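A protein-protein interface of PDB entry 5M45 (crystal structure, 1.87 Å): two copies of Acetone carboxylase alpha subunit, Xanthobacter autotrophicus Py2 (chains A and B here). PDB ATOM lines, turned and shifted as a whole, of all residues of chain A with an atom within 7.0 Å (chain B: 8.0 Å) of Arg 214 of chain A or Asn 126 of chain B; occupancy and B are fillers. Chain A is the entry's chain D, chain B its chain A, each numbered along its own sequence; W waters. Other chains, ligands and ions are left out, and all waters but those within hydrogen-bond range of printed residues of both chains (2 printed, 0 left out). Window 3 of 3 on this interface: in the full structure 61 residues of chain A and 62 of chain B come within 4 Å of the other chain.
A ring nitrogen (ND1) of His 218 of chain A lies within hydrogen-bond range of the side-chain hydroxyl of Tyr 121 of chain B (2.8 Å). The guanidinium group (NE) of Arg 214 of chain A is in hydrogen-bond range of the backbone carbonyl oxygen (O) of Asn 125 of chain B (3.1 Å). The guanidinium group of Arg 214 of chain A lies within hydrogen-bond range of the backbone carbonyl oxygen of Asn 126 of chain B. The side-chain amide nitrogen of Asn 130 of chain B is in hydrogen-bond range of the backbone carbonyl oxygen of Leu 212 of chain A (3.1 Å). The side-chain amide oxygen (OD1) of Asn 130 of chain B is in hydrogen-bond range of the backbone NH (N) of Arg 214 of chain A (2.8 Å). The backbone NH of Thr 202 of chain B sits at hydrogen-bond distance from the side-chain carboxylate of Glu 219 of chain A (3.0 Å). The guanidinium group of Arg 214 of chain A is in salt-bridge range of the side-chain carboxylate of Asp 767 of chain B (3.1 Å). The side-chain carboxylate of Asp 767 of chain B lies within hydrogen-bond range of a ring nitrogen (NE2) of His 218 of chain A (3.0 Å).
No position is printed for both chains. Of the 16 pairs that touch across the chains among the printed residues, none has its exchanged pair printed and touching as well.
Val 206 of chain A touches none of the printed residues of chain B. Of chain B, only Asn 125, Asn 126, Trp 127, Asn 130 and Asp 767 come within 4 Å of Arg 214 of chain A. Ser 220 of chain A touches none of the printed residues of chain B. Asn 126 of chain B touches just one residue of chain A: Arg 214 (3.0 Å). Of the printed residues of chain A, Asn 130 of chain B touches Leu 212, Phe 213 and Arg 214. Printed residues of chain A within 4 Å of Cys 203 of chain B: Asp 215 (3.5 Å). Printed residues of chain A within 4 Å of Arg 204 of chain B: Asp 215. The nearest printed residue of chain A that does not touch Trp 127 of chain B is Trp 216 of chain A (6.1 Å).
Among the printed residues, pairs that only touch across the chains: Phe 213 of chain A with Asn 130 of chain B (3.4 Å), Arg 214 of chain A with Trp 127 of chain B (3.6 Å), Asp 215 of chain A with Trp 127 of chain B (3.7 Å), Asp 215 of chain A with Pro 131 of chain B (3.8 Å), Asp 215 of chain A with Cys 203 of chain B (3.5 Å), Asp 215 of chain A with Arg 204 of chain B (3.4 Å), His 218 of chain A with Asn 125 of chain B (3.5 Å) and His 218 of chain A with Trp 127 of chain B (3.98 Å).
Water W2 bridges the guanidinium group (NH1) of Arg 204 of chain B (2.9 Å) and the side-chain carboxylate (OE1) of Glu 219 of chain A (3.1 Å). Water W1 lies within hydrogen-bond range of the guanidinium group (NH2) of Arg 214 of chain A (3.1 Å) and the side-chain carboxylate (OD1) of Asp 767 of chain B (3.3 Å).
The side-chain amide nitrogen of Asn 125 of chain B sits at hydrogen-bond distance from the backbone carbonyl oxygen of Tyr 121 of chain B (2.9 Å). The indole nitrogen of Trp 127 of chain B is in hydrogen-bond range of the backbone carbonyl oxygen of Cys 203 of chain B (3.0 Å). O of Val 206 of chain A is in hydrogen-bond range of N of Phe 213 of chain A (2.8 Å).
Of the 24 printed residues of chain B, 10 touch a printed residue of chain A. Printed residues of chain B that touch a printed residue of chain A: Tyr 121, Asn 125, Asn 126, Trp 127, Asn 130, Pro 131, Thr 202, Cys 203, Arg 204 and Asp 767. Hydrophobic or aromatic side chains of chain B within 4 Å of the printed part of chain A: Tyr 121, Trp 127 and Pro 131. Of the 11 printed residues of chain A, 6 touch a printed residue of chain B. Hydrophobic or aromatic side chains of chain A within 4 Å of the printed part of chain B: His 218. Among the printed residues, 16 pairs touch across the chains. Among the printed residues, Asp or Glu carboxylates within 4 Å of a Lys or Arg side-chain nitrogen of the other chain: Arg 214 of chain A with Asp 767 of chain B (3.1 Å).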
ATOM      1  N   VAL A 206      20.143 -10.028   6.520  1.00  0.00           N
ATOM      2  CA  VAL A 206      19.437  -9.680   7.754  1.00  0.00           C
ATOM      3  C   VAL A 206      17.924  -9.845   7.692  1.00  0.00           C
ATOM      4  O   VAL A 206      17.225  -9.627   8.696  1.00  0.00           O
ATOM      5  CB  VAL A 206      19.772  -8.226   8.197  1.00  0.00           C
ATOM      6  CG1 VAL A 206      21.291  -8.118   8.489  1.00  0.00           C
ATOM      7  CG2 VAL A 206      19.282  -7.159   7.190  1.00  0.00           C
ATOM      8  N   THR A 211      11.076  -9.269   5.671  1.00  0.00           N
ATOM      9  CA  THR A 211      10.935  -9.292   7.128  1.00  0.00           C
ATOM     10  C   THR A 211      12.319  -9.428   7.775  1.00  0.00           C
ATOM     11  O   THR A 211      13.065 -10.358   7.445  1.00  0.00           O
ATOM     12  CB  THR A 211      10.060 -10.469   7.573  1.00  0.00           C
ATOM     13  OG1 THR A 211       8.823 -10.409   6.860  1.00  0.00           O
ATOM     14  CG2 THR A 211       9.750 -10.429   9.058  1.00  0.00           C
ATOM     15  N   LEU A 212      12.653  -8.508   8.685  1.00  0.00           N
ATOM     16  CA  LEU A 212      13.936  -8.553   9.383  1.00  0.00           C
ATOM     17  C   LEU A 212      14.021  -9.701  10.420  1.00  0.00           C
ATOM     18  O   LEU A 212      13.034  -9.994  11.131  1.00  0.00           O
ATOM     19  CB  LEU A 212      14.235  -7.202  10.059  1.00  0.00           C
ATOM     20  CG  LEU A 212      14.448  -6.020   9.093  1.00  0.00           C
ATOM     21  CD1 LEU A 212      14.420  -4.713   9.898  1.00  0.00           C
ATOM     22  CD2 LEU A 212      15.775  -6.184   8.356  1.00  0.00           C
ATOM     23  N   PHE A 213      15.171 -10.362  10.490  1.00  0.00           N
ATOM     24  CA  PHE A 213      15.328 -11.503  11.404  1.00  0.00           C
ATOM     25  C   PHE A 213      15.516 -11.021  12.852  1.00  0.00           C
ATOM     26  O   PHE A 213      16.275 -10.073  13.107  1.00  0.00           O
ATOM     27  CB  PHE A 213      16.558 -12.365  11.043  1.00  0.00           C
ATOM     28  CG  PHE A 213      16.540 -12.979   9.648  1.00  0.00           C
ATOM     29  CD1 PHE A 213      15.429 -13.552   9.125  1.00  0.00           C
ATOM     30  CD2 PHE A 213      17.721 -13.042   8.910  1.00  0.00           C
ATOM     31  CE1 PHE A 213      15.447 -14.160   7.843  1.00  0.00           C
ATOM     32  CE2 PHE A 213      17.755 -13.630   7.637  1.00  0.00           C
ATOM     33  CZ  PHE A 213      16.620 -14.196   7.109  1.00  0.00           C
ATOM     34  N   ARG A 214      14.874 -11.710  13.803  1.00  0.00           N
ATOM     35  CA  ARG A 214      14.929 -11.291  15.208  1.00  0.00           C
ATOM     36  C   ARG A 214      16.346 -11.362  15.837  1.00  0.00           C
ATOM     37  O   ARG A 214      16.708 -10.504  16.652  1.00  0.00           O
ATOM     38  CB  ARG A 214      13.943 -12.097  16.051  1.00  0.00           C
ATOM     39  CG  ARG A 214      13.607 -11.429  17.380  1.00  0.00           C
ATOM     40  CD  ARG A 214      12.883 -12.353  18.367  1.00  0.00           C
ATOM     41  NE  ARG A 214      11.722 -13.054  17.810  1.00  0.00           N
ATOM     42  CZ  ARG A 214      10.473 -12.590  17.739  1.00  0.00           C
ATOM     43  NH1 ARG A 214       9.541 -13.388  17.221  1.00  0.00           N
ATOM     44  NH2 ARG A 214      10.143 -11.366  18.196  1.00  0.00           N
ATOM     45  N   ASP A 215      17.137 -12.389  15.473  1.00  0.00           N
ATOM     46  CA  ASP A 215      18.526 -12.490  15.979  1.00  0.00           C
ATOM     47  C   ASP A 215      19.367 -11.281  15.581  1.00  0.00           C
ATOM     48  O   ASP A 215      20.110 -10.750  16.413  1.00  0.00           O
ATOM     49  CB  ASP A 215      19.206 -13.834  15.626  1.00  0.00           C
ATOM     50  CG  ASP A 215      19.181 -14.168  14.126  1.00  0.00           C
ATOM     51  OD1 ASP A 215      18.226 -13.761  13.434  1.00  0.00           O
ATOM     52  OD2 ASP A 215      20.127 -14.859  13.651  1.00  0.00           O
ATOM     53  N   TRP A 216      19.219 -10.823  14.340  1.00  0.00           N
ATOM     54  CA  TRP A 216      19.846  -9.558  13.866  1.00  0.00           C
ATOM     55  C   TRP A 216      19.368  -8.347  14.671  1.00  0.00           C
ATOM     56  O   TRP A 216      20.184  -7.523  15.109  1.00  0.00           O
ATOM     57  CB  TRP A 216      19.557  -9.330  12.366  1.00  0.00           C
ATOM     58  CG  TRP A 216      19.664  -7.896  11.905  1.00  0.00           C
ATOM     59  CD1 TRP A 216      18.627  -7.063  11.619  1.00  0.00           C
ATOM     60  CD2 TRP A 216      20.862  -7.123  11.738  1.00  0.00           C
ATOM     61  NE1 TRP A 216      19.099  -5.803  11.257  1.00  0.00           N
ATOM     62  CE2 TRP A 216      20.471  -5.829  11.313  1.00  0.00           C
ATOM     63  CE3 TRP A 216      22.235  -7.406  11.883  1.00  0.00           C
ATOM     64  CZ2 TRP A 216      21.411  -4.813  11.024  1.00  0.00           C
ATOM     65  CZ3 TRP A 216      23.166  -6.389  11.621  1.00  0.00           C
ATOM     66  CH2 TRP A 216      22.751  -5.117  11.166  1.00  0.00           C
ATOM     67  N   LEU A 217      18.047  -8.250  14.870  1.00  0.00           N
ATOM     68  CA  LEU A 217      17.474  -7.107  15.587  1.00  0.00           C
ATOM     69  C   LEU A 217      18.006  -6.997  17.027  1.00  0.00           C
ATOM     70  O   LEU A 217      18.502  -5.930  17.415  1.00  0.00           O
ATOM     71  CB  LEU A 217      15.910  -7.158  15.572  1.00  0.00           C
ATOM     72  CG  LEU A 217      15.228  -6.968  14.206  1.00  0.00           C
ATOM     73  CD1 LEU A 217      13.753  -7.346  14.299  1.00  0.00           C
ATOM     74  CD2 LEU A 217      15.395  -5.539  13.633  1.00  0.00           C
ATOM     75  N   HIS A 218      17.964  -8.110  17.779  1.00  0.00           N
ATOM     76  CA  HIS A 218      18.445  -8.126  19.158  1.00  0.00           C
ATOM     77  C   HIS A 218      19.963  -7.815  19.267  1.00  0.00           C
ATOM     78  O   HIS A 218      20.399  -7.054  20.120  1.00  0.00           O
ATOM     79  CB  HIS A 218      18.100  -9.452  19.873  1.00  0.00           C
ATOM     80  CG  HIS A 218      16.660  -9.600  20.291  1.00  0.00           C
ATOM     81  ND1 HIS A 218      16.285 -10.198  21.482  1.00  0.00           N
ATOM     82  CD2 HIS A 218      15.503  -9.239  19.688  1.00  0.00           C
ATOM     83  CE1 HIS A 218      14.967 -10.172  21.612  1.00  0.00           C
ATOM     84  NE2 HIS A 218      14.463  -9.608  20.538  1.00  0.00           N
ATOM     85  N   GLU A 219      20.759  -8.397  18.381  1.00  0.00           N
ATOM     86  CA  GLU A 219      22.214  -8.220  18.420  1.00  0.00           C
ATOM     87  C   GLU A 219      22.651  -6.789  18.070  1.00  0.00           C
ATOM     88  O   GLU A 219      23.367  -6.126  18.852  1.00  0.00           O
ATOM     89  CB  GLU A 219      22.890  -9.216  17.485  1.00  0.00           C
ATOM     90  CG  GLU A 219      24.402  -9.232  17.564  1.00  0.00           C
ATOM     91  CD  GLU A 219      25.017 -10.198  16.561  1.00  0.00           C
ATOM     92  OE1 GLU A 219      24.993 -11.462  16.830  1.00  0.00           O
ATOM     93  OE2 GLU A 219      25.417  -9.688  15.483  1.00  0.00           O
ATOM     94  N   SER A 220      22.219  -6.326  16.912  1.00  0.00           N
ATOM     95  CA  SER A 220      22.553  -5.017  16.420  1.00  0.00           C
ATOM     96  C   SER A 220      22.191  -3.913  17.424  1.00  0.00           C
ATOM     97  O   SER A 220      23.015  -3.031  17.716  1.00  0.00           O
ATOM     98  CB  SER A 220      21.939  -4.760  15.034  1.00  0.00           C
ATOM     99  OG  SER A 220      20.519  -4.802  15.031  1.00  0.00           O
ATOM    100  N   THR B  23       4.206 -25.088  21.932  1.00  0.00           N
ATOM    101  CA  THR B  23       5.368 -24.219  21.609  1.00  0.00           C
ATOM    102  C   THR B  23       6.487 -24.404  22.664  1.00  0.00           C
ATOM    103  O   THR B  23       6.246 -24.898  23.776  1.00  0.00           O
ATOM    104  CB  THR B  23       5.003 -22.694  21.561  1.00  0.00           C
ATOM    105  OG1 THR B  23       4.612 -22.222  22.870  1.00  0.00           O
ATOM    106  CG2 THR B  23       3.875 -22.433  20.560  1.00  0.00           C
ATOM    107  N   LEU B  24       7.697 -24.004  22.299  1.00  0.00           N
ATOM    108  CA  LEU B  24       8.822 -23.994  23.273  1.00  0.00           C
ATOM    109  C   LEU B  24       8.468 -23.262  24.573  1.00  0.00           C
ATOM    110  O   LEU B  24       8.732 -23.777  25.669  1.00  0.00           O
ATOM    111  CB  LEU B  24      10.089 -23.406  22.647  1.00  0.00           C
ATOM    112  CG  LEU B  24      10.820 -24.233  21.590  1.00  0.00           C
ATOM    113  CD1 LEU B  24      11.823 -23.338  20.870  1.00  0.00           C
ATOM    114  CD2 LEU B  24      11.529 -25.440  22.180  1.00  0.00           C
ATOM    115  N   LYS B  25       7.866 -22.082  24.459  1.00  0.00           N
ATOM    116  CA  LYS B  25       7.508 -21.276  25.647  1.00  0.00           C
ATOM    117  C   LYS B  25       6.379 -21.923  26.468  1.00  0.00           C
ATOM    118  O   LYS B  25       6.469 -21.954  27.689  1.00  0.00           O
ATOM    119  CB  LYS B  25       7.134 -19.828  25.261  1.00  0.00           C
ATOM    120  CG  LYS B  25       6.830 -18.945  26.482  1.00  0.00           C
ATOM    121  CD  LYS B  25       6.764 -17.466  26.152  1.00  0.00           C
ATOM    122  CE  LYS B  25       6.123 -16.622  27.269  1.00  0.00           C
ATOM    123  NZ  LYS B  25       6.779 -16.873  28.588  1.00  0.00           N
ATOM    124  N   LYS B 120      17.216 -20.932  26.784  1.00  0.00           N
ATOM    125  CA  LYS B 120      16.038 -20.362  27.437  1.00  0.00           C
ATOM    126  C   LYS B 120      15.734 -18.914  26.960  1.00  0.00           C
ATOM    127  O   LYS B 120      14.561 -18.520  26.869  1.00  0.00           O
ATOM    128  CB  LYS B 120      16.163 -20.455  28.967  1.00  0.00           C
ATOM    129  CG  LYS B 120      16.128 -21.892  29.476  1.00  0.00           C
ATOM    130  CD  LYS B 120      16.681 -22.063  30.893  1.00  0.00           C
ATOM    131  CE  LYS B 120      16.930 -23.527  31.200  1.00  0.00           C
ATOM    132  NZ  LYS B 120      17.428 -23.763  32.566  1.00  0.00           N
ATOM    133  N   TYR B 121      16.773 -18.130  26.645  1.00  0.00           N
ATOM    134  CA  TYR B 121      16.577 -16.817  26.030  1.00  0.00           C
ATOM    135  C   TYR B 121      15.824 -16.935  24.668  1.00  0.00           C
ATOM    136  O   TYR B 121      14.907 -16.150  24.376  1.00  0.00           O
ATOM    137  CB  TYR B 121      17.915 -16.072  25.849  1.00  0.00           C
ATOM    138  CG  TYR B 121      17.773 -14.641  25.351  1.00  0.00           C
ATOM    139  CD1 TYR B 121      17.549 -13.594  26.246  1.00  0.00           C
ATOM    140  CD2 TYR B 121      17.833 -14.332  23.997  1.00  0.00           C
ATOM    141  CE1 TYR B 121      17.421 -12.281  25.804  1.00  0.00           C
ATOM    142  CE2 TYR B 121      17.713 -13.009  23.539  1.00  0.00           C
ATOM    143  CZ  TYR B 121      17.501 -11.991  24.439  1.00  0.00           C
ATOM    144  OH  TYR B 121      17.355 -10.703  24.026  1.00  0.00           O
ATOM    145  N   MET B 122      16.236 -17.880  23.837  1.00  0.00           N
ATOM    146  CA  MET B 122      15.524 -18.171  22.571  1.00  0.00           C
ATOM    147  C   MET B 122      14.075 -18.572  22.798  1.00  0.00           C
ATOM    148  O   MET B 122      13.160 -18.116  22.085  1.00  0.00           O
ATOM    149  CB  MET B 122      16.271 -19.234  21.717  1.00  0.00           C
ATOM    150  CG  MET B 122      17.667 -18.790  21.233  1.00  0.00           C
ATOM    151  SD  MET B 122      18.430 -19.842  19.975  1.00  0.00           S
ATOM    152  CE  MET B 122      19.135 -21.158  20.933  1.00  0.00           C
ATOM    153  N   ILE B 123      13.848 -19.401  23.795  1.00  0.00           N
ATOM    154  CA  ILE B 123      12.488 -19.836  24.168  1.00  0.00           C
ATOM    155  C   ILE B 123      11.634 -18.615  24.548  1.00  0.00           C
ATOM    156  O   ILE B 123      10.562 -18.386  23.989  1.00  0.00           O
ATOM    157  CB  ILE B 123      12.534 -20.872  25.318  1.00  0.00           C
ATOM    158  CG1 ILE B 123      13.202 -22.155  24.821  1.00  0.00           C
ATOM    159  CG2 ILE B 123      11.117 -21.159  25.833  1.00  0.00           C
ATOM    160  CD1 ILE B 123      13.381 -23.245  25.857  1.00  0.00           C
ATOM    161  N   GLU B 124      12.150 -17.806  25.457  1.00  0.00           N
ATOM    162  CA  GLU B 124      11.420 -16.688  26.037  1.00  0.00           C
ATOM    163  C   GLU B 124      11.224 -15.505  25.088  1.00  0.00           C
ATOM    164  O   GLU B 124      10.323 -14.690  25.299  1.00  0.00           O
ATOM    165  CB  GLU B 124      12.197 -16.223  27.252  1.00  0.00           C
ATOM    166  CG  GLU B 124      11.447 -15.416  28.240  1.00  0.00           C
ATOM    167  CD  GLU B 124      10.278 -16.123  28.955  1.00  0.00           C
ATOM    168  OE1 GLU B 124       9.751 -15.401  29.826  1.00  0.00           O
ATOM    169  OE2 GLU B 124       9.792 -17.278  28.716  1.00  0.00           O
ATOM    170  N   ASN B 125      12.069 -15.377  24.060  1.00  0.00           N
ATOM    171  CA  ASN B 125      11.979 -14.267  23.106  1.00  0.00           C
ATOM    172  C   ASN B 125      11.409 -14.673  21.712  1.00  0.00           C
ATOM    173  O   ASN B 125      11.484 -13.902  20.742  1.00  0.00           O
ATOM    174  CB  ASN B 125      13.331 -13.608  22.979  1.00  0.00           C
ATOM    175  CG  ASN B 125      13.688 -12.815  24.222  1.00  0.00           C
ATOM    176  OD1 ASN B 125      13.344 -11.629  24.317  1.00  0.00           O
ATOM    177  ND2 ASN B 125      14.300 -13.468  25.206  1.00  0.00           N
ATOM    178  N   ASN B 126      10.805 -15.857  21.635  1.00  0.00           N
ATOM    179  CA  ASN B 126      10.034 -16.287  20.466  1.00  0.00           C
ATOM    180  C   ASN B 126      10.880 -16.416  19.192  1.00  0.00           C
ATOM    181  O   ASN B 126      10.438 -16.068  18.073  1.00  0.00           O
ATOM    182  CB  ASN B 126       8.802 -15.406  20.263  1.00  0.00           C
ATOM    183  CG  ASN B 126       7.711 -16.089  19.426  1.00  0.00           C
ATOM    184  OD1 ASN B 126       7.778 -17.264  19.128  1.00  0.00           O
ATOM    185  ND2 ASN B 126       6.679 -15.332  19.092  1.00  0.00           N
ATOM    186  N   TRP B 127      12.068 -16.982  19.364  1.00  0.00           N
ATOM    187  CA  TRP B 127      12.860 -17.473  18.250  1.00  0.00           C
ATOM    188  C   TRP B 127      12.068 -18.478  17.391  1.00  0.00           C
ATOM    189  O   TRP B 127      12.334 -18.601  16.190  1.00  0.00           O
ATOM    190  CB  TRP B 127      14.145 -18.144  18.739  1.00  0.00           C
ATOM    191  CG  TRP B 127      15.432 -17.375  18.566  1.00  0.00           C
ATOM    192  CD1 TRP B 127      16.556 -17.847  17.947  1.00  0.00           C
ATOM    193  CD2 TRP B 127      15.763 -16.067  19.041  1.00  0.00           C
ATOM    194  NE1 TRP B 127      17.551 -16.909  17.974  1.00  0.00           N
ATOM    195  CE2 TRP B 127      17.118 -15.812  18.660  1.00  0.00           C
ATOM    196  CE3 TRP B 127      15.072 -15.079  19.726  1.00  0.00           C
ATOM    197  CZ2 TRP B 127      17.775 -14.613  18.946  1.00  0.00           C
ATOM    198  CZ3 TRP B 127      15.737 -13.869  20.033  1.00  0.00           C
ATOM    199  CH2 TRP B 127      17.082 -13.659  19.623  1.00  0.00           C
ATOM    200  N   GLU B 128      11.119 -19.204  18.009  1.00  0.00           N
ATOM    201  CA  GLU B 128      10.282 -20.158  17.255  1.00  0.00           C
ATOM    202  C   GLU B 128       9.524 -19.487  16.095  1.00  0.00           C
ATOM    203  O   GLU B 128       9.457 -20.071  15.008  1.00  0.00           O
ATOM    204  CB  GLU B 128       9.296 -20.884  18.213  1.00  0.00           C
ATOM    205  CG  GLU B 128       8.364 -21.898  17.571  1.00  0.00           C
ATOM    206  CD  GLU B 128       7.651 -22.791  18.597  1.00  0.00           C
ATOM    207  OE1 GLU B 128       8.014 -22.699  19.819  1.00  0.00           O
ATOM    208  OE2 GLU B 128       6.730 -23.570  18.186  1.00  0.00           O
ATOM    209  N   ALA B 129       8.987 -18.290  16.298  1.00  0.00           N
ATOM    210  CA  ALA B 129       8.266 -17.587  15.235  1.00  0.00           C
ATOM    211  C   ALA B 129       9.212 -16.826  14.283  1.00  0.00           C
ATOM    212  O   ALA B 129       8.874 -16.690  13.125  1.00  0.00           O
ATOM    213  CB  ALA B 129       7.221 -16.632  15.811  1.00  0.00           C
ATOM    214  N   ASN B 130      10.350 -16.313  14.774  1.00  0.00           N
ATOM    215  CA  ASN B 130      11.348 -15.613  13.939  1.00  0.00           C
ATOM    216  C   ASN B 130      12.679 -15.592  14.733  1.00  0.00           C
ATOM    217  O   ASN B 130      12.683 -15.066  15.868  1.00  0.00           O
ATOM    218  CB  ASN B 130      10.841 -14.205  13.643  1.00  0.00           C
ATOM    219  CG  ASN B 130      11.842 -13.324  12.895  1.00  0.00           C
ATOM    220  OD1 ASN B 130      13.007 -13.597  12.796  1.00  0.00           O
ATOM    221  ND2 ASN B 130      11.349 -12.226  12.368  1.00  0.00           N
ATOM    222  N   PRO B 131      13.786 -16.142  14.201  1.00  0.00           N
ATOM    223  CA  PRO B 131      13.958 -16.588  12.792  1.00  0.00           C
ATOM    224  C   PRO B 131      13.530 -18.009  12.474  1.00  0.00           C
ATOM    225  O   PRO B 131      13.797 -18.476  11.353  1.00  0.00           O
ATOM    226  CB  PRO B 131      15.472 -16.474  12.594  1.00  0.00           C
ATOM    227  CG  PRO B 131      16.007 -16.821  13.980  1.00  0.00           C
ATOM    228  CD  PRO B 131      15.046 -16.200  14.947  1.00  0.00           C
ATOM    229  N   GLY B 132      12.857 -18.678  13.419  1.00  0.00           N
ATOM    230  CA  GLY B 132      12.481 -20.089  13.294  1.00  0.00           C
ATOM    231  C   GLY B 132      13.541 -21.027  13.833  1.00  0.00           C
ATOM    232  O   GLY B 132      14.745 -20.707  13.785  1.00  0.00           O
ATOM    233  N   VAL B 133      13.112 -22.194  14.336  1.00  0.00           N
ATOM    234  CA  VAL B 133      14.025 -23.240  14.822  1.00  0.00           C
ATOM    235  C   VAL B 133      13.712 -24.498  14.037  1.00  0.00           C
ATOM    236  O   VAL B 133      12.665 -25.141  14.261  1.00  0.00           O
ATOM    237  CB  VAL B 133      13.862 -23.497  16.347  1.00  0.00           C
ATOM    238  CG1 VAL B 133      14.758 -24.648  16.827  1.00  0.00           C
ATOM    239  CG2 VAL B 133      14.141 -22.221  17.135  1.00  0.00           C
ATOM    240  N   THR B 202      24.659 -12.753  19.471  1.00  0.00           N
ATOM    241  CA  THR B 202      23.458 -13.059  20.273  1.00  0.00           C
ATOM    242  C   THR B 202      22.557 -14.108  19.610  1.00  0.00           C
ATOM    243  O   THR B 202      21.726 -13.759  18.781  1.00  0.00           O
ATOM    244  CB  THR B 202      22.655 -11.775  20.596  1.00  0.00           C
ATOM    245  OG1 THR B 202      23.481 -10.832  21.276  1.00  0.00           O
ATOM    246  CG2 THR B 202      21.422 -12.087  21.481  1.00  0.00           C
ATOM    247  N   CYS B 203      22.740 -15.379  19.970  1.00  0.00           N
ATOM    248  CA  CYS B 203      21.921 -16.502  19.446  1.00  0.00           C
ATOM    249  C   CYS B 203      21.647 -16.398  17.917  1.00  0.00           C
ATOM    250  O   CYS B 203      20.510 -16.539  17.428  1.00  0.00           O
ATOM    251  CB  CYS B 203      20.628 -16.614  20.271  1.00  0.00           C
ATOM    252  SG  CYS B 203      20.889 -17.156  21.988  1.00  0.00           S
ATOM    253  N   ARG B 204      22.735 -16.207  17.161  1.00  0.00           N
ATOM    254  CA  ARG B 204      22.634 -15.990  15.710  1.00  0.00           C
ATOM    255  C   ARG B 204      22.440 -17.315  14.971  1.00  0.00           C
ATOM    256  O   ARG B 204      23.113 -18.301  15.263  1.00  0.00           O
ATOM    257  CB  ARG B 204      23.885 -15.275  15.233  1.00  0.00           C
ATOM    258  CG  ARG B 204      23.958 -15.013  13.716  1.00  0.00           C
ATOM    259  CD  ARG B 204      25.111 -14.106  13.338  1.00  0.00           C
ATOM    260  NE  ARG B 204      25.223 -13.994  11.889  1.00  0.00           N
ATOM    261  CZ  ARG B 204      26.099 -13.199  11.244  1.00  0.00           C
ATOM    262  NH1 ARG B 204      26.931 -12.409  11.912  1.00  0.00           N
ATOM    263  NH2 ARG B 204      26.132 -13.191   9.917  1.00  0.00           N
ATOM    264  N   PRO B 766      13.910  -2.534  23.205  1.00  0.00           N
ATOM    265  CA  PRO B 766      12.619  -3.088  22.730  1.00  0.00           C
ATOM    266  C   PRO B 766      12.654  -4.586  22.424  1.00  0.00           C
ATOM    267  O   PRO B 766      13.670  -5.085  21.876  1.00  0.00           O
ATOM    268  CB  PRO B 766      12.360  -2.306  21.424  1.00  0.00           C
ATOM    269  CG  PRO B 766      13.153  -1.018  21.594  1.00  0.00           C
ATOM    270  CD  PRO B 766      14.388  -1.437  22.343  1.00  0.00           C
ATOM    271  N   ASP B 767      11.563  -5.286  22.748  1.00  0.00           N
ATOM    272  CA  ASP B 767      11.385  -6.737  22.469  1.00  0.00           C
ATOM    273  C   ASP B 767      12.351  -7.671  23.253  1.00  0.00           C
ATOM    274  O   ASP B 767      12.434  -8.847  22.924  1.00  0.00           O
ATOM    275  CB  ASP B 767      11.490  -7.033  20.949  1.00  0.00           C
ATOM    276  CG  ASP B 767      10.958  -8.448  20.545  1.00  0.00           C
ATOM    277  OD1 ASP B 767       9.850  -8.823  21.058  1.00  0.00           O
ATOM    278  OD2 ASP B 767      11.631  -9.153  19.713  1.00  0.00           O
ATOM    279  N   VAL B 768      13.047  -7.175  24.272  1.00  0.00           N
ATOM    280  CA  VAL B 768      13.964  -7.985  25.077  1.00  0.00           C
ATOM    281  C   VAL B 768      13.265  -8.522  26.350  1.00  0.00           C
ATOM    282  O   VAL B 768      12.795  -7.742  27.208  1.00  0.00           O
ATOM    283  CB  VAL B 768      15.239  -7.188  25.463  1.00  0.00           C
ATOM    284  CG1 VAL B 768      16.141  -8.003  26.377  1.00  0.00           C
ATOM    285  CG2 VAL B 768      16.007  -6.773  24.188  1.00  0.00           C
ATOM    286  N   HIS B 769      13.204  -9.845  26.474  1.00  0.00           N
ATOM    287  CA  HIS B 769      12.631 -10.510  27.646  1.00  0.00           C
ATOM    288  C   HIS B 769      13.733 -11.320  28.339  1.00  0.00           C
ATOM    289  O   HIS B 769      14.210 -12.307  27.781  1.00  0.00           O
ATOM    290  CB  HIS B 769      11.524 -11.462  27.203  1.00  0.00           C
ATOM    291  CG  HIS B 769      10.459 -10.809  26.382  1.00  0.00           C
ATOM    292  ND1 HIS B 769      10.613 -10.544  25.027  1.00  0.00           N
ATOM    293  CD2 HIS B 769       9.242 -10.327  26.729  1.00  0.00           C
ATOM    294  CE1 HIS B 769       9.517  -9.952  24.577  1.00  0.00           C
ATOM    295  NE2 HIS B 769       8.679  -9.808  25.591  1.00  0.00           N
HETATM  296  O   HOH W   1       7.560  -9.685  18.777  1.00  0.00           O
HETATM  297  O   HOH W   2      27.265 -12.225  14.809  1.00  0.00           O
